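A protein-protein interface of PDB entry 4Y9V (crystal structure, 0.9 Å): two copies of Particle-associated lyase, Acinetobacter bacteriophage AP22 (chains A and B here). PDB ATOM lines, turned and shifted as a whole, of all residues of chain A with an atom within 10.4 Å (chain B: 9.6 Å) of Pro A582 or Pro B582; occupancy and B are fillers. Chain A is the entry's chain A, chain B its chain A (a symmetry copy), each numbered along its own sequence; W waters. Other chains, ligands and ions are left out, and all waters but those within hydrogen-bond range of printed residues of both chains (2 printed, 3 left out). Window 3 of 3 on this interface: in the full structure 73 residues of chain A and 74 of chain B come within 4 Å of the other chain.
OE1 of Glu A581 is in hydrogen-bond range of N of Lys B607 (2.8 Å).
N of Leu A583 sits at hydrogen-bond distance from O of Asn B605, at 2.8 Å.
The backbone carbonyl oxygen (O) of Pro A582 lies within hydrogen-bond range of the side-chain amino group (NZ) of Lys A606, at 3.2 Å.
The backbone carbonyl oxygen of Pro B582 is in hydrogen-bond range of the side-chain amino group of Lys B606, at 3.2 Å.
O of Lys B606 lies within hydrogen-bond range of NE of Arg B584 (3.0 Å).
The backbone carbonyl oxygen (O) of Lys B607 lies within hydrogen-bond range of the guanidinium group (NH2) of Arg B584 (2.9 Å).
The backbone NH (N) of Thr B585 is in hydrogen-bond range of the side-chain amide oxygen (OD1) of Asn B605, at 2.9 Å.
Thr B537 touches Ala A571.
Glu A581 touches Lys B606 (OE2 to CB, 3.3 Å).
CG of Pro A582 touches CG of Pro B582, 3.9 Å away.
CA of Pro A582 touches O of Asn B605 (3.3 Å).
Leu A583 touches Thr B537.
CB of Leu A583 touches O of Trp B604, 3.4 Å away.
CG2 of Thr A585 touches O of Trp B604, at 3.7 Å.
Asn B605 touches Thr A585.
Asn A605 touches Asn B605 (ND2 to CB, 3.8 Å).
Printed residues of chain B within 4 Å of Ala A571: Thr B537 (3.3 Å).
Leu A583 touches just these residues of chain B: Thr B537, Trp B604 and Asn B605.
Of the printed residues of chain B, Thr A585 touches Trp B604 (3.7 Å) and Asn B605 (3.97 Å).
Glu B576 touches none of the printed residues of chain A.
Of the printed residues of chain A, Pro B582 touches Pro A582.
Leu B583 touches none of the printed residues of chain A.
Printed residues of chain A within 4 Å of Trp B604: Leu A583 (3.4 Å) and Thr A585 (3.7 Å).
Of the printed residues of chain A, Asn B605 touches Pro A582, Leu A583, Thr A585 and Asn A605.
Of the printed residues of chain A, Lys B607 touches Glu A581.
The nearest printed residue of chain B that does not touch Pro A582 is Lys B606 (5.2 Å).
The nearest residue of chain A that does not touch Pro B582 is Glu A581 (6.4 Å).
The nearest printed residue of chain B that does not touch Glu A581 is Asn B605 (4.7 Å).
Hydrophobic or aromatic side chains of chain A within 4 Å of the printed part of chain B: Ala A571, Pro A582 and Leu A583.
Along chain A the printed residues that touch a printed residue of chain B span positions 571 to 605.
Among the printed residues, 11 pairs touch across the chains.
Glu A581 touches Lys B607, but with the chains exchanged Lys A607 does not touch Glu B581 (15.4 Å).
Pro A582 touches Asn B605, but with the chains exchanged Asn A605 does not touch Pro B582 (6.9 Å).
Leu A583 touches Trp B604, but with the chains exchanged Trp A604 does not touch Leu B583 (11.6 Å).
Thr A585 touches Trp B604, but with the chains exchanged Trp A604 does not touch Thr B585 (10.2 Å).
Positions printed for both chains: 571, 574, 575, 576, 577, 578, 579, 580, 581, 582, 583, 584, 585, 604, 605, 606 and 607.
Of the 11 pairs that touch across the chains among the printed residues, 2 have their exchanged pair printed and touching as well.
Water W1 bridges OG1 of Thr B537 and N of Ala A571.
Water W2 bridges the backbone carbonyl oxygen of Lys B607 and the side-chain carboxylate of Glu A581.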
ATOM      1  N   ALA A 571     -27.144  10.898   8.342  1.00  0.00           N
ATOM      2  CA  ALA A 571     -26.781  12.317   8.420  1.00  0.00           C
ATOM      3  C   ALA A 571     -27.965  13.226   8.708  1.00  0.00           C
ATOM      4  O   ALA A 571     -27.735  14.380   9.066  1.00  0.00           O
ATOM      5  CB  ALA A 571     -26.036  12.726   7.165  1.00  0.00           C
ATOM      6  N   PHE A 574     -28.547  14.894  12.730  1.00  0.00           N
ATOM      7  CA  PHE A 574     -27.948  16.123  13.198  1.00  0.00           C
ATOM      8  C   PHE A 574     -27.936  17.251  12.152  1.00  0.00           C
ATOM      9  O   PHE A 574     -27.365  18.301  12.422  1.00  0.00           O
ATOM     10  CB  PHE A 574     -26.511  15.900  13.704  1.00  0.00           C
ATOM     11  CG  PHE A 574     -26.475  15.080  14.993  1.00  0.00           C
ATOM     12  CD1 PHE A 574     -27.040  15.553  16.156  1.00  0.00           C
ATOM     13  CD2 PHE A 574     -25.850  13.833  15.023  1.00  0.00           C
ATOM     14  CE1 PHE A 574     -26.991  14.834  17.339  1.00  0.00           C
ATOM     15  CE2 PHE A 574     -25.828  13.098  16.199  1.00  0.00           C
ATOM     16  CZ  PHE A 574     -26.367  13.595  17.351  1.00  0.00           C
ATOM     17  N   ASN A 575     -28.585  17.024  11.003  1.00  0.00           N
ATOM     18  CA  ASN A 575     -28.619  18.041   9.953  1.00  0.00           C
ATOM     19  C   ASN A 575     -30.031  18.241   9.439  1.00  0.00           C
ATOM     20  O   ASN A 575     -30.709  17.304   9.044  1.00  0.00           O
ATOM     21  CB  ASN A 575     -27.712  17.620   8.753  1.00  0.00           C
ATOM     22  CG  ASN A 575     -26.283  17.687   9.194  1.00  0.00           C
ATOM     23  OD1 ASN A 575     -25.666  18.767   9.229  1.00  0.00           O
ATOM     24  ND2 ASN A 575     -25.741  16.560   9.664  1.00  0.00           N
ATOM     25  N   GLU A 576     -30.386  19.542   9.392  1.00  0.00           N
ATOM     26  CA  GLU A 576     -31.702  19.972   8.886  1.00  0.00           C
ATOM     27  C   GLU A 576     -31.815  19.756   7.376  1.00  0.00           C
ATOM     28  O   GLU A 576     -32.912  19.468   6.877  1.00  0.00           O
ATOM     29  CB  GLU A 576     -31.870  21.458   9.205  1.00  0.00           C
ATOM     30  CG  GLU A 576     -31.980  21.689  10.728  1.00  0.00           C
ATOM     31  CD  GLU A 576     -30.686  21.653  11.543  1.00  0.00           C
ATOM     32  OE1 GLU A 576     -29.601  21.872  10.985  1.00  0.00           O
ATOM     33  OE2 GLU A 576     -30.753  21.446  12.732  1.00  0.00           O
ATOM     34  N   ASP A 577     -30.693  19.827   6.666  1.00  0.00           N
ATOM     35  CA  ASP A 577     -30.643  19.645   5.222  1.00  0.00           C
ATOM     36  C   ASP A 577     -29.287  19.050   4.939  1.00  0.00           C
ATOM     37  O   ASP A 577     -28.264  19.684   5.082  1.00  0.00           O
ATOM     38  CB  ASP A 577     -30.774  20.979   4.494  1.00  0.00           C
ATOM     39  CG  ASP A 577     -30.785  20.860   2.998  1.00  0.00           C
ATOM     40  OD1 ASP A 577     -30.361  19.829   2.462  1.00  0.00           O
ATOM     41  OD2 ASP A 577     -31.205  21.843   2.362  1.00  0.00           O
ATOM     42  N   THR A 578     -29.243  17.747   4.525  1.00  0.00           N
ATOM     43  CA  THR A 578     -27.985  17.092   4.319  1.00  0.00           C
ATOM     44  C   THR A 578     -27.273  17.555   3.058  1.00  0.00           C
ATOM     45  O   THR A 578     -26.116  17.140   2.867  1.00  0.00           O
ATOM     46  CB  THR A 578     -28.135  15.554   4.312  1.00  0.00           C
ATOM     47  OG1 THR A 578     -29.078  15.247   3.274  1.00  0.00           O
ATOM     48  CG2 THR A 578     -28.670  15.066   5.638  1.00  0.00           C
ATOM     49  N   ASN A 579     -27.842  18.412   2.249  1.00  0.00           N
ATOM     50  CA  ASN A 579     -27.215  19.042   1.113  1.00  0.00           C
ATOM     51  C   ASN A 579     -26.316  20.186   1.575  1.00  0.00           C
ATOM     52  O   ASN A 579     -25.461  20.610   0.796  1.00  0.00           O
ATOM     53  CB  ASN A 579     -28.223  19.678   0.159  1.00  0.00           C
ATOM     54  CG  ASN A 579     -29.043  18.710  -0.643  1.00  0.00           C
ATOM     55  OD1 ASN A 579     -28.760  17.541  -0.751  1.00  0.00           O
ATOM     56  ND2 ASN A 579     -30.073  19.360  -1.222  1.00  0.00           N
ATOM     57  N   VAL A 580     -26.549  20.671   2.787  1.00  0.00           N
ATOM     58  CA  VAL A 580     -25.800  21.855   3.296  1.00  0.00           C
ATOM     59  C   VAL A 580     -24.599  21.373   4.051  1.00  0.00           C
ATOM     60  O   VAL A 580     -24.709  20.633   5.055  1.00  0.00           O
ATOM     61  CB  VAL A 580     -26.650  22.712   4.236  1.00  0.00           C
ATOM     62  CG1 VAL A 580     -25.857  23.770   4.986  1.00  0.00           C
ATOM     63  CG2 VAL A 580     -27.730  23.429   3.442  1.00  0.00           C
ATOM     64  N   GLU A 581     -23.391  21.794   3.538  1.00  0.00           N
ATOM     65  CA  GLU A 581     -22.101  21.453   4.065  1.00  0.00           C
ATOM     66  C   GLU A 581     -21.326  22.670   4.550  1.00  0.00           C
ATOM     67  O   GLU A 581     -21.579  23.779   4.036  1.00  0.00           O
ATOM     68  CB  GLU A 581     -21.181  20.750   3.059  1.00  0.00           C
ATOM     69  CG  GLU A 581     -21.898  19.424   2.586  1.00  0.00           C
ATOM     70  CD  GLU A 581     -20.915  18.481   1.916  1.00  0.00           C
ATOM     71  OE1 GLU A 581     -21.265  17.292   1.874  1.00  0.00           O
ATOM     72  OE2 GLU A 581     -19.782  18.778   1.505  1.00  0.00           O
ATOM     73  N   PRO A 582     -20.461  22.539   5.573  1.00  0.00           N
ATOM     74  CA  PRO A 582     -20.180  21.322   6.338  1.00  0.00           C
ATOM     75  C   PRO A 582     -21.418  20.759   7.004  1.00  0.00           C
ATOM     76  O   PRO A 582     -22.340  21.479   7.399  1.00  0.00           O
ATOM     77  CB  PRO A 582     -19.201  21.847   7.414  1.00  0.00           C
ATOM     78  CG  PRO A 582     -18.906  23.245   7.074  1.00  0.00           C
ATOM     79  CD  PRO A 582     -19.730  23.744   6.000  1.00  0.00           C
ATOM     80  N   LEU A 583     -21.413  19.444   7.155  1.00  0.00           N
ATOM     81  CA  LEU A 583     -22.431  18.718   7.903  1.00  0.00           C
ATOM     82  C   LEU A 583     -22.048  18.733   9.387  1.00  0.00           C
ATOM     83  O   LEU A 583     -20.894  18.534   9.745  1.00  0.00           O
ATOM     84  CB  LEU A 583     -22.499  17.293   7.426  1.00  0.00           C
ATOM     85  CG  LEU A 583     -23.027  17.144   5.988  1.00  0.00           C
ATOM     86  CD1 LEU A 583     -22.445  15.931   5.325  1.00  0.00           C
ATOM     87  CD2 LEU A 583     -24.552  17.211   5.959  1.00  0.00           C
ATOM     88  N   ARG A 584     -23.064  18.981  10.237  1.00  0.00           N
ATOM     89  CA  ARG A 584     -22.889  18.927  11.679  1.00  0.00           C
ATOM     90  C   ARG A 584     -22.647  17.476  12.133  1.00  0.00           C
ATOM     91  O   ARG A 584     -23.383  16.588  11.734  1.00  0.00           O
ATOM     92  CB  ARG A 584     -24.151  19.466  12.335  1.00  0.00           C
ATOM     93  CG  ARG A 584     -24.063  19.571  13.856  1.00  0.00           C
ATOM     94  CD  ARG A 584     -25.292  20.181  14.449  1.00  0.00           C
ATOM     95  NE  ARG A 584     -25.538  21.575  14.082  1.00  0.00           N
ATOM     96  CZ  ARG A 584     -26.373  21.998  13.127  1.00  0.00           C
ATOM     97  NH1 ARG A 584     -27.032  21.160  12.310  1.00  0.00           N
ATOM     98  NH2 ARG A 584     -26.526  23.297  12.953  1.00  0.00           N
ATOM     99  N   THR A 585     -21.629  17.336  12.998  1.00  0.00           N
ATOM    100  CA  THR A 585     -21.358  16.019  13.596  1.00  0.00           C
ATOM    101  C   THR A 585     -21.043  16.226  15.074  1.00  0.00           C
ATOM    102  O   THR A 585     -20.609  17.312  15.492  1.00  0.00           O
ATOM    103  CB  THR A 585     -20.253  15.213  12.933  1.00  0.00           C
ATOM    104  OG1 THR A 585     -19.075  15.874  13.324  1.00  0.00           O
ATOM    105  CG2 THR A 585     -20.316  15.188  11.419  1.00  0.00           C
ATOM    106  N   TRP A 604     -19.459  20.590  19.016  1.00  0.00           N
ATOM    107  CA  TRP A 604     -20.103  20.713  17.718  1.00  0.00           C
ATOM    108  C   TRP A 604     -19.217  21.462  16.733  1.00  0.00           C
ATOM    109  O   TRP A 604     -18.609  22.492  17.109  1.00  0.00           O
ATOM    110  CB  TRP A 604     -21.454  21.465  17.849  1.00  0.00           C
ATOM    111  CG  TRP A 604     -22.413  20.766  18.750  1.00  0.00           C
ATOM    112  CD1 TRP A 604     -22.771  21.139  20.008  1.00  0.00           C
ATOM    113  CD2 TRP A 604     -23.144  19.556  18.450  1.00  0.00           C
ATOM    114  NE1 TRP A 604     -23.682  20.234  20.535  1.00  0.00           N
ATOM    115  CE2 TRP A 604     -23.909  19.264  19.602  1.00  0.00           C
ATOM    116  CE3 TRP A 604     -23.204  18.707  17.365  1.00  0.00           C
ATOM    117  CZ2 TRP A 604     -24.742  18.132  19.674  1.00  0.00           C
ATOM    118  CZ3 TRP A 604     -24.024  17.578  17.414  1.00  0.00           C
ATOM    119  CH2 TRP A 604     -24.776  17.319  18.580  1.00  0.00           C
ATOM    120  N   ASN A 605     -19.201  21.049  15.492  1.00  0.00           N
ATOM    121  CA  ASN A 605     -18.541  21.831  14.441  1.00  0.00           C
ATOM    122  C   ASN A 605     -19.399  22.957  13.902  1.00  0.00           C
ATOM    123  O   ASN A 605     -18.868  23.850  13.248  1.00  0.00           O
ATOM    124  CB  ASN A 605     -18.023  20.925  13.306  1.00  0.00           C
ATOM    125  CG  ASN A 605     -19.125  20.136  12.622  1.00  0.00           C
ATOM    126  OD1 ASN A 605     -20.125  19.754  13.231  1.00  0.00           O
ATOM    127  ND2 ASN A 605     -18.915  19.861  11.336  1.00  0.00           N
ATOM    128  N   LYS A 606     -20.686  22.982  14.130  1.00  0.00           N
ATOM    129  CA  LYS A 606     -21.465  24.201  13.840  1.00  0.00           C
ATOM    130  C   LYS A 606     -22.601  24.121  14.862  1.00  0.00           C
ATOM    131  O   LYS A 606     -23.184  23.074  15.167  1.00  0.00           O
ATOM    132  CB  LYS A 606     -21.897  24.363  12.392  1.00  0.00           C
ATOM    133  CG  LYS A 606     -22.809  23.284  11.909  1.00  0.00           C
ATOM    134  CD  LYS A 606     -23.616  23.743  10.723  1.00  0.00           C
ATOM    135  CE  LYS A 606     -24.183  22.722   9.798  1.00  0.00           C
ATOM    136  NZ  LYS A 606     -24.777  23.298   8.536  1.00  0.00           N
ATOM    137  N   LYS A 607     -22.894  25.311  15.377  1.00  0.00           N
ATOM    138  CA  LYS A 607     -23.740  25.472  16.530  1.00  0.00           C
ATOM    139  C   LYS A 607     -25.125  24.898  16.232  1.00  0.00           C
ATOM    140  O   LYS A 607     -25.650  24.943  15.114  1.00  0.00           O
ATOM    141  CB  LYS A 607     -23.830  26.910  17.015  1.00  0.00           C
ATOM    142  CG  LYS A 607     -24.706  27.849  16.359  1.00  0.00           C
ATOM    143  CD  LYS A 607     -24.642  29.241  16.993  1.00  0.00           C
ATOM    144  CE  LYS A 607     -25.384  30.221  16.055  1.00  0.00           C
ATOM    145  NZ  LYS A 607     -25.377  31.544  16.687  1.00  0.00           N
ATOM    146  N   VAL A 609     -28.984  24.082  15.865  1.00  0.00           N
ATOM    147  CA  VAL A 609     -30.218  24.710  15.450  1.00  0.00           C
ATOM    148  C   VAL A 609     -31.428  23.957  15.975  1.00  0.00           C
ATOM    149  O   VAL A 609     -32.425  24.580  16.317  1.00  0.00           O
ATOM    150  CB  VAL A 609     -30.228  24.859  13.923  1.00  0.00           C
ATOM    151  CG1 VAL A 609     -31.617  25.286  13.419  1.00  0.00           C
ATOM    152  CG2 VAL A 609     -29.170  25.821  13.435  1.00  0.00           C
ATOM    153  N   THR B 537     -22.665  10.560   3.254  1.00  0.00           N
ATOM    154  CA  THR B 537     -22.692  11.496   4.364  1.00  0.00           C
ATOM    155  C   THR B 537     -22.565  10.759   5.695  1.00  0.00           C
ATOM    156  O   THR B 537     -22.275  11.372   6.728  1.00  0.00           O
ATOM    157  CB  THR B 537     -23.945  12.365   4.307  1.00  0.00           C
ATOM    158  OG1 THR B 537     -25.078  11.471   4.263  1.00  0.00           O
ATOM    159  CG2 THR B 537     -23.930  13.288   3.080  1.00  0.00           C
ATOM    160  N   ALA B 571      -3.552  13.781   7.625  1.00  0.00           N
ATOM    161  CA  ALA B 571      -4.727  14.422   7.024  1.00  0.00           C
ATOM    162  C   ALA B 571      -4.932  14.054   5.563  1.00  0.00           C
ATOM    163  O   ALA B 571      -6.021  14.306   5.050  1.00  0.00           O
ATOM    164  CB  ALA B 571      -4.656  15.922   7.234  1.00  0.00           C
ATOM    165  N   PHE B 574      -8.034  11.158   4.426  1.00  0.00           N
ATOM    166  CA  PHE B 574      -9.412  11.502   4.161  1.00  0.00           C
ATOM    167  C   PHE B 574      -9.590  12.809   3.371  1.00  0.00           C
ATOM    168  O   PHE B 574     -10.724  13.233   3.179  1.00  0.00           O
ATOM    169  CB  PHE B 574     -10.236  11.589   5.458  1.00  0.00           C
ATOM    170  CG  PHE B 574     -10.426  10.222   6.115  1.00  0.00           C
ATOM    171  CD1 PHE B 574     -11.125   9.218   5.484  1.00  0.00           C
ATOM    172  CD2 PHE B 574      -9.902   9.966   7.382  1.00  0.00           C
ATOM    173  CE1 PHE B 574     -11.327   7.983   6.078  1.00  0.00           C
ATOM    174  CE2 PHE B 574     -10.078   8.720   7.965  1.00  0.00           C
ATOM    175  CZ  PHE B 574     -10.800   7.745   7.339  1.00  0.00           C
ATOM    176  N   ASN B 575      -8.480  13.399   2.908  1.00  0.00           N
ATOM    177  CA  ASN B 575      -8.559  14.647   2.151  1.00  0.00           C
ATOM    178  C   ASN B 575      -7.728  14.566   0.886  1.00  0.00           C
ATOM    179  O   ASN B 575      -6.549  14.245   0.914  1.00  0.00           O
ATOM    180  CB  ASN B 575      -8.038  15.843   3.010  1.00  0.00           C
ATOM    181  CG  ASN B 575      -9.019  16.094   4.114  1.00  0.00           C
ATOM    182  OD1 ASN B 575     -10.061  16.743   3.918  1.00  0.00           O
ATOM    183  ND2 ASN B 575      -8.783  15.488   5.281  1.00  0.00           N
ATOM    184  N   GLU B 576      -8.406  14.969  -0.208  1.00  0.00           N
ATOM    185  CA  GLU B 576      -7.779  15.012  -1.542  1.00  0.00           C
ATOM    186  C   GLU B 576      -6.732  16.123  -1.628  1.00  0.00           C
ATOM    187  O   GLU B 576      -5.731  15.969  -2.341  1.00  0.00           O
ATOM    188  CB  GLU B 576      -8.879  15.263  -2.574  1.00  0.00           C
ATOM    189  CG  GLU B 576      -9.836  14.055  -2.669  1.00  0.00           C
ATOM    190  CD  GLU B 576     -10.891  13.903  -1.571  1.00  0.00           C
ATOM    191  OE1 GLU B 576     -11.247  14.894  -0.918  1.00  0.00           O
ATOM    192  OE2 GLU B 576     -11.387  12.816  -1.388  1.00  0.00           O
ATOM    193  N   ASP B 577      -6.921  17.198  -0.867  1.00  0.00           N
ATOM    194  CA  ASP B 577      -6.011  18.334  -0.842  1.00  0.00           C
ATOM    195  C   ASP B 577      -6.103  18.892   0.555  1.00  0.00           C
ATOM    196  O   ASP B 577      -7.103  19.444   0.962  1.00  0.00           O
ATOM    197  CB  ASP B 577      -6.439  19.403  -1.844  1.00  0.00           C
ATOM    198  CG  ASP B 577      -5.514  20.582  -1.912  1.00  0.00           C
ATOM    199  OD1 ASP B 577      -4.722  20.794  -0.985  1.00  0.00           O
ATOM    200  OD2 ASP B 577      -5.616  21.318  -2.909  1.00  0.00           O
ATOM    201  N   THR B 578      -5.015  18.741   1.369  1.00  0.00           N
ATOM    202  CA  THR B 578      -5.062  19.172   2.735  1.00  0.00           C
ATOM    203  C   THR B 578      -5.008  20.683   2.884  1.00  0.00           C
ATOM    204  O   THR B 578      -5.178  21.154   4.023  1.00  0.00           O
ATOM    205  CB  THR B 578      -3.951  18.513   3.582  1.00  0.00           C
ATOM    206  OG1 THR B 578      -2.708  18.859   2.953  1.00  0.00           O
ATOM    207  CG2 THR B 578      -4.109  17.010   3.591  1.00  0.00           C
ATOM    208  N   ASN B 579      -4.859  21.451   1.835  1.00  0.00           N
ATOM    209  CA  ASN B 579      -4.946  22.891   1.824  1.00  0.00           C
ATOM    210  C   ASN B 579      -6.409  23.329   1.844  1.00  0.00           C
ATOM    211  O   ASN B 579      -6.668  24.488   2.171  1.00  0.00           O
ATOM    212  CB  ASN B 579      -4.355  23.509   0.560  1.00  0.00           C
ATOM    213  CG  ASN B 579      -2.859  23.452   0.461  1.00  0.00           C
ATOM    214  OD1 ASN B 579      -2.147  23.200   1.403  1.00  0.00           O
ATOM    215  ND2 ASN B 579      -2.476  23.760  -0.795  1.00  0.00           N
ATOM    216  N   VAL B 580      -7.305  22.426   1.468  1.00  0.00           N
ATOM    217  CA  VAL B 580      -8.747  22.779   1.351  1.00  0.00           C
ATOM    218  C   VAL B 580      -9.425  22.463   2.650  1.00  0.00           C
ATOM    219  O   VAL B 580      -9.436  21.302   3.117  1.00  0.00           O
ATOM    220  CB  VAL B 580      -9.444  21.991   0.240  1.00  0.00           C
ATOM    221  CG1 VAL B 580     -10.960  22.115   0.257  1.00  0.00           C
ATOM    222  CG2 VAL B 580      -8.962  22.481  -1.117  1.00  0.00           C
ATOM    223  N   GLU B 581     -10.000  23.548   3.275  1.00  0.00           N
ATOM    224  CA  GLU B 581     -10.687  23.511   4.535  1.00  0.00           C
ATOM    225  C   GLU B 581     -12.151  23.908   4.415  1.00  0.00           C
ATOM    226  O   GLU B 581     -12.488  24.662   3.479  1.00  0.00           O
ATOM    227  CB  GLU B 581     -10.090  24.442   5.598  1.00  0.00           C
ATOM    228  CG  GLU B 581      -8.587  24.017   5.833  1.00  0.00           C
ATOM    229  CD  GLU B 581      -8.049  24.604   7.125  1.00  0.00           C
ATOM    230  OE1 GLU B 581      -7.055  24.028   7.595  1.00  0.00           O
ATOM    231  OE2 GLU B 581      -8.563  25.525   7.780  1.00  0.00           O
ATOM    232  N   PRO B 582     -13.053  23.372   5.259  1.00  0.00           N
ATOM    233  CA  PRO B 582     -12.798  22.380   6.306  1.00  0.00           C
ATOM    234  C   PRO B 582     -12.197  21.102   5.760  1.00  0.00           C
ATOM    235  O   PRO B 582     -12.462  20.680   4.631  1.00  0.00           O
ATOM    236  CB  PRO B 582     -14.227  22.104   6.831  1.00  0.00           C
ATOM    237  CG  PRO B 582     -15.119  23.053   6.153  1.00  0.00           C
ATOM    238  CD  PRO B 582     -14.457  23.793   5.107  1.00  0.00           C
ATOM    239  N   LEU B 583     -11.398  20.465   6.602  1.00  0.00           N
ATOM    240  CA  LEU B 583     -10.840  19.146   6.334  1.00  0.00           C
ATOM    241  C   LEU B 583     -11.868  18.089   6.754  1.00  0.00           C
ATOM    242  O   LEU B 583     -12.489  18.191   7.805  1.00  0.00           O
ATOM    243  CB  LEU B 583      -9.580  18.952   7.132  1.00  0.00           C
ATOM    244  CG  LEU B 583      -8.419  19.860   6.690  1.00  0.00           C
ATOM    245  CD1 LEU B 583      -7.509  20.169   7.841  1.00  0.00           C
ATOM    246  CD2 LEU B 583      -7.714  19.282   5.464  1.00  0.00           C
ATOM    247  N   ARG B 584     -12.023  17.069   5.888  1.00  0.00           N
ATOM    248  CA  ARG B 584     -12.880  15.933   6.185  1.00  0.00           C
ATOM    249  C   ARG B 584     -12.274  15.090   7.322  1.00  0.00           C
ATOM    250  O   ARG B 584     -11.098  14.767   7.273  1.00  0.00           O
ATOM    251  CB  ARG B 584     -13.005  15.084   4.929  1.00  0.00           C
ATOM    252  CG  ARG B 584     -13.971  13.910   5.067  1.00  0.00           C
ATOM    253  CD  ARG B 584     -14.124  13.155   3.785  1.00  0.00           C
ATOM    254  NE  ARG B 584     -14.739  13.903   2.689  1.00  0.00           N
ATOM    255  CZ  ARG B 584     -14.086  14.510   1.692  1.00  0.00           C
ATOM    256  NH1 ARG B 584     -12.747  14.583   1.634  1.00  0.00           N
ATOM    257  NH2 ARG B 584     -14.791  15.100   0.745  1.00  0.00           N
ATOM    258  N   THR B 585     -13.155  14.743   8.275  1.00  0.00           N
ATOM    259  CA  THR B 585     -12.732  13.846   9.363  1.00  0.00           C
ATOM    260  C   THR B 585     -13.854  12.841   9.609  1.00  0.00           C
ATOM    261  O   THR B 585     -15.029  13.101   9.302  1.00  0.00           O
ATOM    262  CB  THR B 585     -12.350  14.531  10.665  1.00  0.00           C
ATOM    263  OG1 THR B 585     -13.581  14.953  11.198  1.00  0.00           O
ATOM    264  CG2 THR B 585     -11.453  15.741  10.497  1.00  0.00           C
ATOM    265  N   TRP B 604     -19.767  11.959   8.452  1.00  0.00           N
ATOM    266  CA  TRP B 604     -18.812  12.810   7.761  1.00  0.00           C
ATOM    267  C   TRP B 604     -19.191  14.280   7.889  1.00  0.00           C
ATOM    268  O   TRP B 604     -20.388  14.623   7.748  1.00  0.00           O
ATOM    269  CB  TRP B 604     -18.743  12.441   6.255  1.00  0.00           C
ATOM    270  CG  TRP B 604     -18.317  11.031   6.031  1.00  0.00           C
ATOM    271  CD1 TRP B 604     -19.102   9.994   5.631  1.00  0.00           C
ATOM    272  CD2 TRP B 604     -16.982  10.503   6.196  1.00  0.00           C
ATOM    273  NE1 TRP B 604     -18.351   8.831   5.540  1.00  0.00           N
ATOM    274  CE2 TRP B 604     -17.064   9.125   5.889  1.00  0.00           C
ATOM    275  CE3 TRP B 604     -15.772  11.039   6.585  1.00  0.00           C
ATOM    276  CZ2 TRP B 604     -15.941   8.281   5.961  1.00  0.00           C
ATOM    277  CZ3 TRP B 604     -14.645  10.219   6.662  1.00  0.00           C
ATOM    278  CH2 TRP B 604     -14.763   8.847   6.346  1.00  0.00           C
ATOM    279  N   ASN B 605     -18.224  15.145   8.050  1.00  0.00           N
ATOM    280  CA  ASN B 605     -18.477  16.588   7.977  1.00  0.00           C
ATOM    281  C   ASN B 605     -18.520  17.119   6.559  1.00  0.00           C
ATOM    282  O   ASN B 605     -19.010  18.226   6.353  1.00  0.00           O
ATOM    283  CB  ASN B 605     -17.479  17.380   8.845  1.00  0.00           C
ATOM    284  CG  ASN B 605     -16.034  17.180   8.425  1.00  0.00           C
ATOM    285  OD1 ASN B 605     -15.638  16.118   7.945  1.00  0.00           O
ATOM    286  ND2 ASN B 605     -15.227  18.217   8.646  1.00  0.00           N
ATOM    287  N   LYS B 606     -18.047  16.411   5.568  1.00  0.00           N
ATOM    288  CA  LYS B 606     -18.330  16.807   4.175  1.00  0.00           C
ATOM    289  C   LYS B 606     -18.304  15.467   3.436  1.00  0.00           C
ATOM    290  O   LYS B 606     -17.490  14.566   3.669  1.00  0.00           O
ATOM    291  CB  LYS B 606     -17.419  17.884   3.611  1.00  0.00           C
ATOM    292  CG  LYS B 606     -15.983  17.483   3.537  1.00  0.00           C
ATOM    293  CD  LYS B 606     -15.238  18.307   2.519  1.00  0.00           C
ATOM    294  CE  LYS B 606     -13.760  18.434   2.638  1.00  0.00           C
ATOM    295  NZ  LYS B 606     -13.153  19.454   1.705  1.00  0.00           N
ATOM    296  N   LYS B 607     -19.253  15.389   2.509  1.00  0.00           N
ATOM    297  CA  LYS B 607     -19.603  14.155   1.857  1.00  0.00           C
ATOM    298  C   LYS B 607     -18.383  13.605   1.117  1.00  0.00           C
ATOM    299  O   LYS B 607     -17.533  14.327   0.583  1.00  0.00           O
ATOM    300  CB  LYS B 607     -20.800  14.282   0.929  1.00  0.00           C
ATOM    301  CG  LYS B 607     -20.643  14.829  -0.396  1.00  0.00           C
ATOM    302  CD  LYS B 607     -21.968  14.879  -1.162  1.00  0.00           C
ATOM    303  CE  LYS B 607     -21.745  15.729  -2.434  1.00  0.00           C
ATOM    304  NZ  LYS B 607     -22.995  15.731  -3.202  1.00  0.00           N
HETATM  305  O   HOH W   1     -26.475   9.639   5.847  1.00  0.00           O
HETATM  306  O   HOH W   2     -17.857  17.085  -0.313  1.00  0.00           O
